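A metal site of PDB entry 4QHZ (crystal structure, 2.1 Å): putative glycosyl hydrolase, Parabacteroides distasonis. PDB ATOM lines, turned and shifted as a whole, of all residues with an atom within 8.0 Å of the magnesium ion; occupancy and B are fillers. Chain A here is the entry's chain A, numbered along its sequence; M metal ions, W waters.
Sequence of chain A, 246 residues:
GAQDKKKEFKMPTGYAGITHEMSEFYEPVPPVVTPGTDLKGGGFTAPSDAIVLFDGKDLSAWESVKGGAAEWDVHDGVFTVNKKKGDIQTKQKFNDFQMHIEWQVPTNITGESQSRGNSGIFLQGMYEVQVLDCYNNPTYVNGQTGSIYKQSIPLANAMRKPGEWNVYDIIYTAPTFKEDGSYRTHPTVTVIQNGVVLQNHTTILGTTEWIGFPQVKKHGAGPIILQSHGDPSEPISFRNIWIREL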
ATOM      1  N   GLN A 114      25.936  30.979 -13.289  1.00  0.00           N
ATOM      2  CA  GLN A 114      25.176  30.111 -14.192  1.00  0.00           C
ATOM      3  C   GLN A 114      25.912  29.744 -15.481  1.00  0.00           C
ATOM      4  O   GLN A 114      25.413  28.919 -16.248  1.00  0.00           O
ATOM      5  CB  GLN A 114      23.843  30.772 -14.569  1.00  0.00           C
ATOM      6  CG  GLN A 114      22.929  31.013 -13.370  1.00  0.00           C
ATOM      7  CD  GLN A 114      22.321  29.728 -12.807  1.00  0.00           C
ATOM      8  OE1 GLN A 114      21.727  28.950 -13.545  1.00  0.00           O
ATOM      9  NE2 GLN A 114      22.485  29.511 -11.504  1.00  0.00           N
ATOM     10  N   GLY A 117      29.559  25.127 -16.480  1.00  0.00           N
ATOM     11  CA  GLY A 117      29.101  23.754 -16.499  1.00  0.00           C
ATOM     12  C   GLY A 117      27.604  23.597 -16.341  1.00  0.00           C
ATOM     13  O   GLY A 117      27.130  22.659 -15.687  1.00  0.00           O
ATOM     14  N   ASN A 118      26.847  24.518 -16.946  1.00  0.00           N
ATOM     15  CA  ASN A 118      25.395  24.503 -16.884  1.00  0.00           C
ATOM     16  C   ASN A 118      24.792  23.503 -17.871  1.00  0.00           C
ATOM     17  O   ASN A 118      25.036  23.589 -19.081  1.00  0.00           O
ATOM     18  CB  ASN A 118      24.823  25.895 -17.161  1.00  0.00           C
ATOM     19  CG  ASN A 118      23.353  26.051 -16.766  1.00  0.00           C
ATOM     20  OD1 ASN A 118      22.589  25.084 -16.731  1.00  0.00           O
ATOM     21  ND2 ASN A 118      22.955  27.283 -16.457  1.00  0.00           N
ATOM     22  N   SER A 119      24.066  22.535 -17.337  1.00  0.00           N
ATOM     23  CA  SER A 119      23.184  21.688 -18.121  1.00  0.00           C
ATOM     24  C   SER A 119      21.922  21.511 -17.285  1.00  0.00           C
ATOM     25  O   SER A 119      21.593  22.372 -16.475  1.00  0.00           O
ATOM     26  CB  SER A 119      23.844  20.355 -18.457  1.00  0.00           C
ATOM     27  OG  SER A 119      22.999  19.565 -19.296  1.00  0.00           O
ATOM     28  N   GLY A 120      21.227  20.409 -17.479  1.00  0.00           N
ATOM     29  CA  GLY A 120      20.030  20.155 -16.700  1.00  0.00           C
ATOM     30  C   GLY A 120      19.243  18.983 -17.225  1.00  0.00           C
ATOM     31  O   GLY A 120      19.388  18.587 -18.381  1.00  0.00           O
ATOM     32  N   ILE A 121      18.424  18.409 -16.348  1.00  0.00           N
ATOM     33  CA  ILE A 121      17.552  17.307 -16.690  1.00  0.00           C
ATOM     34  C   ILE A 121      16.102  17.801 -16.614  1.00  0.00           C
ATOM     35  O   ILE A 121      15.601  18.089 -15.529  1.00  0.00           O
ATOM     36  CB  ILE A 121      17.765  16.117 -15.737  1.00  0.00           C
ATOM     37  CG1 ILE A 121      19.225  15.660 -15.791  1.00  0.00           C
ATOM     38  CG2 ILE A 121      16.854  14.960 -16.088  1.00  0.00           C
ATOM     39  CD1 ILE A 121      19.979  15.901 -14.505  1.00  0.00           C
ATOM     40  N   PHE A 122      15.466  17.948 -17.770  1.00  0.00           N
ATOM     41  CA  PHE A 122      14.074  18.386 -17.828  1.00  0.00           C
ATOM     42  C   PHE A 122      13.155  17.175 -17.729  1.00  0.00           C
ATOM     43  O   PHE A 122      13.041  16.389 -18.675  1.00  0.00           O
ATOM     44  CB  PHE A 122      13.784  19.167 -19.101  1.00  0.00           C
ATOM     45  CG  PHE A 122      14.275  20.586 -19.079  1.00  0.00           C
ATOM     46  CD1 PHE A 122      15.615  20.876 -19.259  1.00  0.00           C
ATOM     47  CD2 PHE A 122      13.385  21.635 -18.893  1.00  0.00           C
ATOM     48  CE1 PHE A 122      16.065  22.184 -19.246  1.00  0.00           C
ATOM     49  CE2 PHE A 122      13.826  22.947 -18.877  1.00  0.00           C
ATOM     50  CZ  PHE A 122      15.168  23.215 -19.053  1.00  0.00           C
ATOM     51  N   GLU A 128      13.062  21.457 -14.893  1.00  0.00           N
ATOM     52  CA  GLU A 128      14.515  21.288 -14.865  1.00  0.00           C
ATOM     53  C   GLU A 128      15.045  20.999 -13.477  1.00  0.00           C
ATOM     54  O   GLU A 128      14.836  21.773 -12.548  1.00  0.00           O
ATOM     55  CB  GLU A 128      15.242  22.531 -15.412  1.00  0.00           C
ATOM     56  CG  GLU A 128      16.752  22.299 -15.507  1.00  0.00           C
ATOM     57  CD  GLU A 128      17.548  23.508 -15.972  1.00  0.00           C
ATOM     58  OE1 GLU A 128      16.991  24.631 -16.019  1.00  0.00           O
ATOM     59  OE2 GLU A 128      18.744  23.335 -16.302  1.00  0.00           O
ATOM     60  N   VAL A 129      15.751  19.873 -13.359  1.00  0.00           N
ATOM     61  CA  VAL A 129      16.672  19.640 -12.261  1.00  0.00           C
ATOM     62  C   VAL A 129      18.010  20.193 -12.707  1.00  0.00           C
ATOM     63  O   VAL A 129      18.615  19.675 -13.648  1.00  0.00           O
ATOM     64  CB  VAL A 129      16.800  18.154 -11.914  1.00  0.00           C
ATOM     65  CG1 VAL A 129      17.721  17.974 -10.721  1.00  0.00           C
ATOM     66  CG2 VAL A 129      15.427  17.551 -11.630  1.00  0.00           C
ATOM     67  N   GLN A 130      18.459  21.258 -12.058  1.00  0.00           N
ATOM     68  CA  GLN A 130      19.642  21.977 -12.489  1.00  0.00           C
ATOM     69  C   GLN A 130      20.905  21.144 -12.386  1.00  0.00           C
ATOM     70  O   GLN A 130      21.100  20.415 -11.415  1.00  0.00           O
ATOM     71  CB  GLN A 130      19.796  23.277 -11.681  1.00  0.00           C
ATOM     72  CG  GLN A 130      21.034  24.106 -11.981  1.00  0.00           C
ATOM     73  CD  GLN A 130      21.005  24.789 -13.345  1.00  0.00           C
ATOM     74  OE1 GLN A 130      20.874  24.127 -14.375  1.00  0.00           O
ATOM     75  NE2 GLN A 130      21.144  26.113 -13.347  1.00  0.00           N
ATOM     76  N   VAL A 131      21.734  21.249 -13.416  1.00  0.00           N
ATOM     77  CA  VAL A 131      23.099  20.743 -13.389  1.00  0.00           C
ATOM     78  C   VAL A 131      24.023  21.950 -13.564  1.00  0.00           C
ATOM     79  O   VAL A 131      23.827  22.768 -14.468  1.00  0.00           O
ATOM     80  CB  VAL A 131      23.306  19.709 -14.500  1.00  0.00           C
ATOM     81  CG1 VAL A 131      24.795  19.407 -14.701  1.00  0.00           C
ATOM     82  CG2 VAL A 131      22.544  18.436 -14.159  1.00  0.00           C
ATOM     83  N   LEU A 132      25.020  22.062 -12.698  1.00  0.00           N
ATOM     84  CA  LEU A 132      25.923  23.190 -12.690  1.00  0.00           C
ATOM     85  C   LEU A 132      27.157  22.859 -11.860  1.00  0.00           C
ATOM     86  O   LEU A 132      27.069  22.082 -10.899  1.00  0.00           O
ATOM     87  CB  LEU A 132      25.219  24.414 -12.116  1.00  0.00           C
ATOM     88  CG  LEU A 132      25.880  25.778 -12.231  1.00  0.00           C
ATOM     89  CD1 LEU A 132      26.003  26.203 -13.686  1.00  0.00           C
ATOM     90  CD2 LEU A 132      25.073  26.807 -11.448  1.00  0.00           C
ATOM     91  N   GLY A 143      18.722  28.599  -8.064  1.00  0.00           N
ATOM     92  CA  GLY A 143      19.120  28.068  -9.366  1.00  0.00           C
ATOM     93  C   GLY A 143      20.448  27.322  -9.365  1.00  0.00           C
ATOM     94  O   GLY A 143      21.037  27.118 -10.429  1.00  0.00           O
ATOM     95  N   GLN A 144      20.924  26.918  -8.193  1.00  0.00           N
ATOM     96  CA  GLN A 144      22.194  26.207  -8.117  1.00  0.00           C
ATOM     97  C   GLN A 144      21.970  24.708  -8.342  1.00  0.00           C
ATOM     98  O   GLN A 144      20.838  24.259  -8.577  1.00  0.00           O
ATOM     99  CB  GLN A 144      22.925  26.511  -6.804  1.00  0.00           C
ATOM    100  CG  GLN A 144      22.448  25.761  -5.570  1.00  0.00           C
ATOM    101  CD  GLN A 144      23.221  26.191  -4.338  1.00  0.00           C
ATOM    102  OE1 GLN A 144      23.211  27.365  -3.976  1.00  0.00           O
ATOM    103  NE2 GLN A 144      23.888  25.243  -3.679  1.00  0.00           N
ATOM    104  N   SER A 147      18.795  22.208  -7.720  1.00  0.00           N
ATOM    105  CA  SER A 147      17.567  22.970  -7.553  1.00  0.00           C
ATOM    106  C   SER A 147      16.537  22.459  -8.552  1.00  0.00           C
ATOM    107  O   SER A 147      16.900  21.902  -9.594  1.00  0.00           O
ATOM    108  CB  SER A 147      17.805  24.464  -7.779  1.00  0.00           C
ATOM    109  OG  SER A 147      18.206  24.752  -9.109  1.00  0.00           O
ATOM    110  N   TYR A 149      14.743  24.278 -10.875  1.00  0.00           N
ATOM    111  CA  TYR A 149      15.290  25.573 -11.272  1.00  0.00           C
ATOM    112  C   TYR A 149      14.374  26.774 -10.959  1.00  0.00           C
ATOM    113  O   TYR A 149      13.275  26.876 -11.496  1.00  0.00           O
ATOM    114  CB  TYR A 149      15.654  25.558 -12.753  1.00  0.00           C
ATOM    115  CG  TYR A 149      16.314  26.841 -13.225  1.00  0.00           C
ATOM    116  CD1 TYR A 149      17.592  27.165 -12.817  1.00  0.00           C
ATOM    117  CD2 TYR A 149      15.645  27.720 -14.061  1.00  0.00           C
ATOM    118  CE1 TYR A 149      18.204  28.346 -13.243  1.00  0.00           C
ATOM    119  CE2 TYR A 149      16.245  28.897 -14.482  1.00  0.00           C
ATOM    120  CZ  TYR A 149      17.517  29.203 -14.069  1.00  0.00           C
ATOM    121  OH  TYR A 149      18.107  30.367 -14.506  1.00  0.00           O
ATOM    122  N   GLN A 227      19.974  19.473 -21.252  1.00  0.00           N
ATOM    123  CA  GLN A 227      20.119  20.859 -21.683  1.00  0.00           C
ATOM    124  C   GLN A 227      21.500  21.168 -22.241  1.00  0.00           C
ATOM    125  O   GLN A 227      22.520  20.840 -21.634  1.00  0.00           O
ATOM    126  CB  GLN A 227      19.824  21.793 -20.504  1.00  0.00           C
ATOM    127  CG  GLN A 227      19.876  23.288 -20.812  1.00  0.00           C
ATOM    128  CD  GLN A 227      19.764  24.113 -19.539  1.00  0.00           C
ATOM    129  OE1 GLN A 227      20.543  23.939 -18.602  1.00  0.00           O
ATOM    130  NE2 GLN A 227      18.780  24.997 -19.492  1.00  0.00           N
ATOM    131  N   SER A 228      21.512  21.806 -23.417  1.00  0.00           N
ATOM    132  CA  SER A 228      22.682  22.451 -23.958  1.00  0.00           C
ATOM    133  C   SER A 228      22.568  23.938 -23.659  1.00  0.00           C
ATOM    134  O   SER A 228      21.879  24.659 -24.351  1.00  0.00           O
ATOM    135  CB  SER A 228      22.770  22.213 -25.459  1.00  0.00           C
ATOM    136  OG  SER A 228      23.825  22.961 -26.028  1.00  0.00           O
ATOM    137  N   HIS A 229      23.231  24.378 -22.598  1.00  0.00           N
ATOM    138  CA  HIS A 229      23.161  25.778 -22.167  1.00  0.00           C
ATOM    139  C   HIS A 229      24.237  26.576 -22.902  1.00  0.00           C
ATOM    140  O   HIS A 229      25.431  26.318 -22.735  1.00  0.00           O
ATOM    141  CB  HIS A 229      23.325  25.876 -20.651  1.00  0.00           C
ATOM    142  CG  HIS A 229      22.934  27.199 -20.086  1.00  0.00           C
ATOM    143  ND1 HIS A 229      23.843  28.203 -19.831  1.00  0.00           N
ATOM    144  CD2 HIS A 229      21.723  27.685 -19.708  1.00  0.00           C
ATOM    145  CE1 HIS A 229      23.208  29.250 -19.338  1.00  0.00           C
ATOM    146  NE2 HIS A 229      21.919  28.967 -19.250  1.00  0.00           N
ATOM    147  N   ASP A 231      26.125  29.114 -22.958  1.00  0.00           N
ATOM    148  CA  ASP A 231      27.259  29.884 -22.458  1.00  0.00           C
ATOM    149  C   ASP A 231      28.568  29.261 -22.966  1.00  0.00           C
ATOM    150  O   ASP A 231      28.582  28.119 -23.431  1.00  0.00           O
ATOM    151  CB  ASP A 231      27.234  29.951 -20.920  1.00  0.00           C
ATOM    152  CG  ASP A 231      27.515  28.612 -20.277  1.00  0.00           C
ATOM    153  OD1 ASP A 231      28.684  28.204 -20.221  1.00  0.00           O
ATOM    154  OD2 ASP A 231      26.549  27.961 -19.819  1.00  0.00           O
HETATM  155 MG    MG M   1      20.629  24.216 -16.523  1.00  0.00          MG
HETATM  156  O   HOH W   1      19.582  25.931 -16.412  1.00  0.00           O
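The magnesium ion is bound by water W1 (2.0 Å), O of Ser 119 (2.1 Å), OE2 of Glu 128 (2.1 Å), OE1 of Gln 227 (2.1 Å), OD1 of Asn 118 (2.2 Å) and OE1 of Gln 130 (2.2 Å).
Water W1 lies within hydrogen-bond range of OE1 of Glu 128, NE2 of Gln 227 and NE2 of Gln 130.
Merely in contact with the magnesium ion: Gly 120 (3.97 Å).
Six residues have an atom within 4 Å of the magnesium ion: Asn 118, Ser 119, Gly 120, Glu 128, Gln 130 and Gln 227.
The nearest printed residue that does not touch the magnesium ion is Val 131 (4.1 Å).
O of Val 131 sits at hydrogen-bond distance from N of Ser 119.
N of Tyr 149 is in hydrogen-bond range of O of Glu 128, 3.0 Å away.
The side-chain amide oxygen (OD1) of Asn 118 sits close to the backbone carbonyl oxygen (O) of Val 131 (3.5 Å).
The side-chain amide nitrogen of Asn 118 lies within hydrogen-bond range of a ring nitrogen (NE2) of His 229, at 3.4 Å.
The backbone carbonyl oxygen (O) of Gln 114 lies within hydrogen-bond range of the side-chain amide nitrogen (ND2) of Asn 118.
The side-chain amide nitrogen of Gln 130 sits at hydrogen-bond distance from the side-chain amide oxygen of Gln 114 (2.9 Å).
The side-chain amide nitrogen (NE2) of Gln 130 lies within hydrogen-bond range of the backbone carbonyl oxygen (O) of Gly 143.
The backbone NH (N) of Gln 130 lies within hydrogen-bond range of the backbone carbonyl oxygen (O) of Ser 147, at 3.0 Å.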
